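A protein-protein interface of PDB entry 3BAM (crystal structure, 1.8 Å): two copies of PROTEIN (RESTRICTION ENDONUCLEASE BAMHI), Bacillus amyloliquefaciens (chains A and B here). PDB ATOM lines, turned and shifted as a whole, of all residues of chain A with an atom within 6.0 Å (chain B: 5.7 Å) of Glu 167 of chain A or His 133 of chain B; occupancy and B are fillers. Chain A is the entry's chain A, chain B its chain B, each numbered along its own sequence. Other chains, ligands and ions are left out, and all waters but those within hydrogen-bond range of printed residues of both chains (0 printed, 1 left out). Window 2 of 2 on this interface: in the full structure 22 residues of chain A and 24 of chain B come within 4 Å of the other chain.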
ATOM      1  N   PHE A   7     -18.625 -12.885  -8.674  1.00  0.00           N
ATOM      2  CA  PHE A   7     -19.382 -12.811  -7.438  1.00  0.00           C
ATOM      3  C   PHE A   7     -20.218 -14.077  -7.354  1.00  0.00           C
ATOM      4  O   PHE A   7     -20.997 -14.369  -8.257  1.00  0.00           O
ATOM      5  CB  PHE A   7     -20.294 -11.585  -7.368  1.00  0.00           C
ATOM      6  CG  PHE A   7     -21.128 -11.549  -6.120  1.00  0.00           C
ATOM      7  CD1 PHE A   7     -22.483 -11.842  -6.165  1.00  0.00           C
ATOM      8  CD2 PHE A   7     -20.533 -11.318  -4.884  1.00  0.00           C
ATOM      9  CE1 PHE A   7     -23.235 -11.913  -5.000  1.00  0.00           C
ATOM     10  CE2 PHE A   7     -21.274 -11.387  -3.712  1.00  0.00           C
ATOM     11  CZ  PHE A   7     -22.632 -11.687  -3.772  1.00  0.00           C
ATOM     12  N   GLU A 163     -23.211  -4.718 -10.537  1.00  0.00           N
ATOM     13  CA  GLU A 163     -22.754  -5.085  -9.207  1.00  0.00           C
ATOM     14  C   GLU A 163     -23.584  -4.563  -8.029  1.00  0.00           C
ATOM     15  O   GLU A 163     -23.983  -5.347  -7.171  1.00  0.00           O
ATOM     16  CB  GLU A 163     -21.276  -4.731  -9.039  1.00  0.00           C
ATOM     17  CG  GLU A 163     -20.663  -5.247  -7.750  1.00  0.00           C
ATOM     18  CD  GLU A 163     -19.152  -5.102  -7.711  1.00  0.00           C
ATOM     19  OE1 GLU A 163     -18.579  -4.342  -8.535  1.00  0.00           O
ATOM     20  OE2 GLU A 163     -18.530  -5.759  -6.849  1.00  0.00           O
ATOM     21  N   PRO A 164     -23.891  -3.255  -7.986  1.00  0.00           N
ATOM     22  CA  PRO A 164     -24.685  -2.776  -6.854  1.00  0.00           C
ATOM     23  C   PRO A 164     -26.027  -3.488  -6.677  1.00  0.00           C
ATOM     24  O   PRO A 164     -26.620  -3.437  -5.608  1.00  0.00           O
ATOM     25  CB  PRO A 164     -24.852  -1.282  -7.154  1.00  0.00           C
ATOM     26  CG  PRO A 164     -24.647  -1.180  -8.619  1.00  0.00           C
ATOM     27  CD  PRO A 164     -23.539  -2.141  -8.880  1.00  0.00           C
ATOM     28  N   TYR A 165     -26.478  -4.198  -7.702  1.00  0.00           N
ATOM     29  CA  TYR A 165     -27.745  -4.914  -7.633  1.00  0.00           C
ATOM     30  C   TYR A 165     -27.590  -6.409  -7.378  1.00  0.00           C
ATOM     31  O   TYR A 165     -28.588  -7.107  -7.230  1.00  0.00           O
ATOM     32  CB  TYR A 165     -28.555  -4.698  -8.919  1.00  0.00           C
ATOM     33  CG  TYR A 165     -28.974  -3.261  -9.145  1.00  0.00           C
ATOM     34  CD1 TYR A 165     -30.195  -2.789  -8.679  1.00  0.00           C
ATOM     35  CD2 TYR A 165     -28.126  -2.363  -9.785  1.00  0.00           C
ATOM     36  CE1 TYR A 165     -30.557  -1.452  -8.841  1.00  0.00           C
ATOM     37  CE2 TYR A 165     -28.478  -1.024  -9.949  1.00  0.00           C
ATOM     38  CZ  TYR A 165     -29.694  -0.579  -9.474  1.00  0.00           C
ATOM     39  OH  TYR A 165     -30.047   0.734  -9.628  1.00  0.00           O
ATOM     40  N   PHE A 166     -26.358  -6.900  -7.272  1.00  0.00           N
ATOM     41  CA  PHE A 166     -26.140  -8.327  -7.031  1.00  0.00           C
ATOM     42  C   PHE A 166     -26.883  -8.786  -5.779  1.00  0.00           C
ATOM     43  O   PHE A 166     -27.385  -9.908  -5.731  1.00  0.00           O
ATOM     44  CB  PHE A 166     -24.652  -8.644  -6.853  1.00  0.00           C
ATOM     45  CG  PHE A 166     -23.844  -8.562  -8.118  1.00  0.00           C
ATOM     46  CD1 PHE A 166     -24.444  -8.293  -9.338  1.00  0.00           C
ATOM     47  CD2 PHE A 166     -22.470  -8.791  -8.085  1.00  0.00           C
ATOM     48  CE1 PHE A 166     -23.681  -8.222 -10.496  1.00  0.00           C
ATOM     49  CE2 PHE A 166     -21.703  -8.723  -9.239  1.00  0.00           C
ATOM     50  CZ  PHE A 166     -22.313  -8.451 -10.448  1.00  0.00           C
ATOM     51  N   GLU A 167     -26.977  -7.912  -4.778  1.00  0.00           N
ATOM     52  CA  GLU A 167     -27.655  -8.247  -3.526  1.00  0.00           C
ATOM     53  C   GLU A 167     -29.133  -8.643  -3.665  1.00  0.00           C
ATOM     54  O   GLU A 167     -29.702  -9.244  -2.760  1.00  0.00           O
ATOM     55  CB  GLU A 167     -27.502  -7.124  -2.502  1.00  0.00           C
ATOM     56  CG  GLU A 167     -28.211  -5.835  -2.858  1.00  0.00           C
ATOM     57  CD  GLU A 167     -28.470  -4.977  -1.644  1.00  0.00           C
ATOM     58  OE1 GLU A 167     -29.598  -5.038  -1.118  1.00  0.00           O
ATOM     59  OE2 GLU A 167     -27.554  -4.250  -1.205  1.00  0.00           O
ATOM     60  N   LEU A 168     -29.747  -8.340  -4.801  1.00  0.00           N
ATOM     61  CA  LEU A 168     -31.141  -8.705  -5.022  1.00  0.00           C
ATOM     62  C   LEU A 168     -31.309 -10.208  -5.248  1.00  0.00           C
ATOM     63  O   LEU A 168     -32.423 -10.696  -5.406  1.00  0.00           O
ATOM     64  CB  LEU A 168     -31.712  -7.920  -6.199  1.00  0.00           C
ATOM     65  CG  LEU A 168     -31.810  -6.413  -5.958  1.00  0.00           C
ATOM     66  CD1 LEU A 168     -32.346  -5.744  -7.213  1.00  0.00           C
ATOM     67  CD2 LEU A 168     -32.712  -6.134  -4.757  1.00  0.00           C
ATOM     68  N   THR A 169     -30.199 -10.939  -5.290  1.00  0.00           N
ATOM     69  CA  THR A 169     -30.247 -12.385  -5.475  1.00  0.00           C
ATOM     70  C   THR A 169     -29.966 -13.120  -4.171  1.00  0.00           C
ATOM     71  O   THR A 169     -29.729 -14.326  -4.168  1.00  0.00           O
ATOM     72  CB  THR A 169     -29.242 -12.857  -6.526  1.00  0.00           C
ATOM     73  OG1 THR A 169     -27.912 -12.634  -6.046  1.00  0.00           O
ATOM     74  CG2 THR A 169     -29.449 -12.096  -7.823  1.00  0.00           C
ATOM     75  N   GLU A 170     -29.981 -12.388  -3.060  1.00  0.00           N
ATOM     76  CA  GLU A 170     -29.741 -12.974  -1.746  1.00  0.00           C
ATOM     77  C   GLU A 170     -30.661 -14.165  -1.525  1.00  0.00           C
ATOM     78  O   GLU A 170     -31.864 -14.086  -1.788  1.00  0.00           O
ATOM     79  CB  GLU A 170     -30.001 -11.950  -0.643  1.00  0.00           C
ATOM     80  CG  GLU A 170     -28.923 -10.892  -0.469  1.00  0.00           C
ATOM     81  CD  GLU A 170     -29.310  -9.847   0.568  1.00  0.00           C
ATOM     82  OE1 GLU A 170     -29.663  -8.712   0.174  1.00  0.00           O
ATOM     83  OE2 GLU A 170     -29.269 -10.160   1.779  1.00  0.00           O
ATOM     84  N   ILE B  82     -27.918   4.001  -0.203  1.00  0.00           N
ATOM     85  CA  ILE B  82     -27.220   2.752  -0.472  1.00  0.00           C
ATOM     86  C   ILE B  82     -26.430   2.788  -1.783  1.00  0.00           C
ATOM     87  O   ILE B  82     -25.365   2.185  -1.875  1.00  0.00           O
ATOM     88  CB  ILE B  82     -28.178   1.538  -0.472  1.00  0.00           C
ATOM     89  CG1 ILE B  82     -27.356   0.254  -0.589  1.00  0.00           C
ATOM     90  CG2 ILE B  82     -29.245   1.667  -1.573  1.00  0.00           C
ATOM     91  CD1 ILE B  82     -28.133  -0.964  -0.989  1.00  0.00           C
ATOM     92  N   GLU B  86     -23.217   4.426   0.150  1.00  0.00           N
ATOM     93  CA  GLU B  86     -22.655   3.113   0.444  1.00  0.00           C
ATOM     94  C   GLU B  86     -21.869   2.488  -0.709  1.00  0.00           C
ATOM     95  O   GLU B  86     -20.642   2.387  -0.653  1.00  0.00           O
ATOM     96  CB  GLU B  86     -23.738   2.151   0.932  1.00  0.00           C
ATOM     97  CG  GLU B  86     -23.172   0.866   1.509  1.00  0.00           C
ATOM     98  CD  GLU B  86     -24.212  -0.214   1.686  1.00  0.00           C
ATOM     99  OE1 GLU B  86     -25.364   0.115   2.053  1.00  0.00           O
ATOM    100  OE2 GLU B  86     -23.874  -1.397   1.452  1.00  0.00           O
ATOM    101  N   LYS B  87     -22.577   2.056  -1.744  1.00  0.00           N
ATOM    102  CA  LYS B  87     -21.950   1.432  -2.897  1.00  0.00           C
ATOM    103  C   LYS B  87     -21.355   2.414  -3.894  1.00  0.00           C
ATOM    104  O   LYS B  87     -20.640   2.003  -4.800  1.00  0.00           O
ATOM    105  CB  LYS B  87     -22.951   0.519  -3.596  1.00  0.00           C
ATOM    106  CG  LYS B  87     -23.408  -0.608  -2.703  1.00  0.00           C
ATOM    107  CD  LYS B  87     -24.461  -1.474  -3.351  1.00  0.00           C
ATOM    108  CE  LYS B  87     -24.767  -2.667  -2.457  1.00  0.00           C
ATOM    109  NZ  LYS B  87     -25.734  -3.605  -3.073  1.00  0.00           N
ATOM    110  N   LEU B 128     -36.827  -1.208  -5.605  1.00  0.00           N
ATOM    111  CA  LEU B 128     -36.821  -2.375  -4.736  1.00  0.00           C
ATOM    112  C   LEU B 128     -35.658  -2.284  -3.747  1.00  0.00           C
ATOM    113  O   LEU B 128     -35.829  -2.559  -2.561  1.00  0.00           O
ATOM    114  CB  LEU B 128     -36.715  -3.627  -5.602  1.00  0.00           C
ATOM    115  CG  LEU B 128     -37.481  -4.887  -5.219  1.00  0.00           C
ATOM    116  CD1 LEU B 128     -38.848  -4.542  -4.659  1.00  0.00           C
ATOM    117  CD2 LEU B 128     -37.609  -5.767  -6.449  1.00  0.00           C
ATOM    118  N   LEU B 129     -34.500  -1.832  -4.226  1.00  0.00           N
ATOM    119  CA  LEU B 129     -33.306  -1.677  -3.403  1.00  0.00           C
ATOM    120  C   LEU B 129     -33.562  -0.616  -2.325  1.00  0.00           C
ATOM    121  O   LEU B 129     -33.186  -0.797  -1.160  1.00  0.00           O
ATOM    122  CB  LEU B 129     -32.126  -1.266  -4.294  1.00  0.00           C
ATOM    123  CG  LEU B 129     -30.697  -1.649  -3.905  1.00  0.00           C
ATOM    124  CD1 LEU B 129     -30.561  -3.152  -3.751  1.00  0.00           C
ATOM    125  CD2 LEU B 129     -29.752  -1.148  -4.975  1.00  0.00           C
ATOM    126  N   GLY B 130     -34.198   0.487  -2.725  1.00  0.00           N
ATOM    127  CA  GLY B 130     -34.526   1.567  -1.804  1.00  0.00           C
ATOM    128  C   GLY B 130     -35.488   1.104  -0.731  1.00  0.00           C
ATOM    129  O   GLY B 130     -35.350   1.471   0.438  1.00  0.00           O
ATOM    130  N   LEU B 131     -36.494   0.343  -1.151  1.00  0.00           N
ATOM    131  CA  LEU B 131     -37.498  -0.230  -0.264  1.00  0.00           C
ATOM    132  C   LEU B 131     -36.853  -1.205   0.721  1.00  0.00           C
ATOM    133  O   LEU B 131     -37.032  -1.087   1.934  1.00  0.00           O
ATOM    134  CB  LEU B 131     -38.554  -0.962  -1.080  1.00  0.00           C
ATOM    135  CG  LEU B 131     -39.707  -0.143  -1.643  1.00  0.00           C
ATOM    136  CD1 LEU B 131     -40.448  -0.954  -2.702  1.00  0.00           C
ATOM    137  CD2 LEU B 131     -40.624   0.300  -0.507  1.00  0.00           C
ATOM    138  N   LYS B 132     -36.074  -2.150   0.203  1.00  0.00           N
ATOM    139  CA  LYS B 132     -35.410  -3.119   1.060  1.00  0.00           C
ATOM    140  C   LYS B 132     -34.476  -2.444   2.052  1.00  0.00           C
ATOM    141  O   LYS B 132     -34.227  -2.980   3.122  1.00  0.00           O
ATOM    142  CB  LYS B 132     -34.654  -4.154   0.228  1.00  0.00           C
ATOM    143  CG  LYS B 132     -35.568  -5.019  -0.640  1.00  0.00           C
ATOM    144  CD  LYS B 132     -34.786  -6.117  -1.365  1.00  0.00           C
ATOM    145  CE  LYS B 132     -35.685  -6.945  -2.294  1.00  0.00           C
ATOM    146  NZ  LYS B 132     -36.756  -7.679  -1.571  1.00  0.00           N
ATOM    147  N   HIS B 133     -33.943  -1.278   1.699  1.00  0.00           N
ATOM    148  CA  HIS B 133     -33.052  -0.575   2.601  1.00  0.00           C
ATOM    149  C   HIS B 133     -33.729   0.493   3.459  1.00  0.00           C
ATOM    150  O   HIS B 133     -33.062   1.303   4.108  1.00  0.00           O
ATOM    151  CB  HIS B 133     -31.836  -0.046   1.843  1.00  0.00           C
ATOM    152  CG  HIS B 133     -30.844  -1.119   1.512  1.00  0.00           C
ATOM    153  ND1 HIS B 133     -29.702  -1.331   2.253  1.00  0.00           N
ATOM    154  CD2 HIS B 133     -30.866  -2.094   0.575  1.00  0.00           C
ATOM    155  CE1 HIS B 133     -29.066  -2.390   1.795  1.00  0.00           C
ATOM    156  NE2 HIS B 133     -29.753  -2.875   0.774  1.00  0.00           N
ATOM    157  N   GLY B 134     -35.056   0.452   3.487  1.00  0.00           N
ATOM    158  CA  GLY B 134     -35.830   1.376   4.291  1.00  0.00           C
ATOM    159  C   GLY B 134     -35.668   2.840   3.969  1.00  0.00           C
ATOM    160  O   GLY B 134     -35.729   3.677   4.862  1.00  0.00           O
ATOM    161  N   GLU B 135     -35.450   3.156   2.701  1.00  0.00           N
ATOM    162  CA  GLU B 135     -35.286   4.543   2.295  1.00  0.00           C
ATOM    163  C   GLU B 135     -36.584   5.136   1.757  1.00  0.00           C
ATOM    164  O   GLU B 135     -36.744   6.351   1.732  1.00  0.00           O
ATOM    165  CB  GLU B 135     -34.149   4.677   1.284  1.00  0.00           C
ATOM    166  CG  GLU B 135     -32.797   4.318   1.876  1.00  0.00           C
ATOM    167  CD  GLU B 135     -31.646   4.802   1.040  1.00  0.00           C
ATOM    168  OE1 GLU B 135     -30.720   4.009   0.790  1.00  0.00           O
ATOM    169  OE2 GLU B 135     -31.654   5.986   0.639  1.00  0.00           O
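The side-chain amino group of Lys 87 of chain B lies within hydrogen-bond range of the backbone carbonyl oxygen of Pro 164 of chain A (2.7 Å).
The side-chain carboxylate (OE2) of Glu 167 of chain A lies within salt-bridge range of the side-chain amino group (NZ) of Lys 87 of chain B (2.7 Å).
A ring nitrogen (NE2) of His 133 of chain B lies within hydrogen-bond range of the side-chain carboxylate (OE1) of Glu 167 of chain A, at 2.9 Å.
O of Ile 82 of chain B is in hydrogen-bond range of N of Lys 87 of chain B.
N of Ile 82 of chain B is in hydrogen-bond range of OE1 of Glu 135 of chain B (3.0 Å).
Among the printed residues, pairs that only touch across the chains: Glu 167 of chain A with Ile 82 of chain B (3.3 Å), Glu 167 of chain A with Leu 129 of chain B (3.4 Å), Leu 168 of chain A with Leu 129 of chain B (3.8 Å), Pro 164 of chain A with Leu 129 of chain B (3.9 Å), Leu 168 of chain A with Lys 132 of chain B (3.9 Å) and Tyr 165 of chain A with Leu 129 of chain B (3.96 Å).
Glu 167 of chain A touches just these residues of chain B: Ile 82, Lys 87, Leu 129 and His 133.
His 133 of chain B touches one residue of chain A.
Of the printed residues of chain B, Tyr 165 of chain A touches Leu 129.
Of the printed residues of chain A, Leu 129 of chain B touches Pro 164 (3.9 Å), Tyr 165 (3.96 Å), Glu 167 (3.4 Å) and Leu 168 (3.8 Å).
Printed residues of chain A within 4 Å of Lys 87 of chain B: Pro 164 and Glu 167.
Of the printed residues of chain A, Ile 82 of chain B touches Glu 167.
Printed residues of chain B within 4 Å of Pro 164 of chain A: Lys 87 and Leu 129.
Glu 86 of chain B touches none of the printed residues of chain A.
Thr 169 of chain A touches none of the printed residues of chain B.
The nearest residue of chain B that does not touch Glu 167 of chain A is Lys 132 of chain B (5.3 Å).
The nearest residue of chain A that does not touch His 133 of chain B is Glu 170 of chain A (5.9 Å).
Printed residues of chain B that touch a printed residue of chain A: Ile 82, Lys 87, Leu 129, Lys 132 and His 133.
Along chain B the printed residues that touch a printed residue of chain A span positions 82 to 133.
Among the printed residues, 9 pairs touch across the chains.
Among the printed residues, Asp or Glu carboxylates within 4 Å of a Lys or Arg side-chain nitrogen of the other chain: Glu 167 of chain A with Lys 87 of chain B (2.7 Å).
No position is printed for both chains.
Of the 9 pairs that touch across the chains among the printed residues, none has its exchanged pair printed and touching as well.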
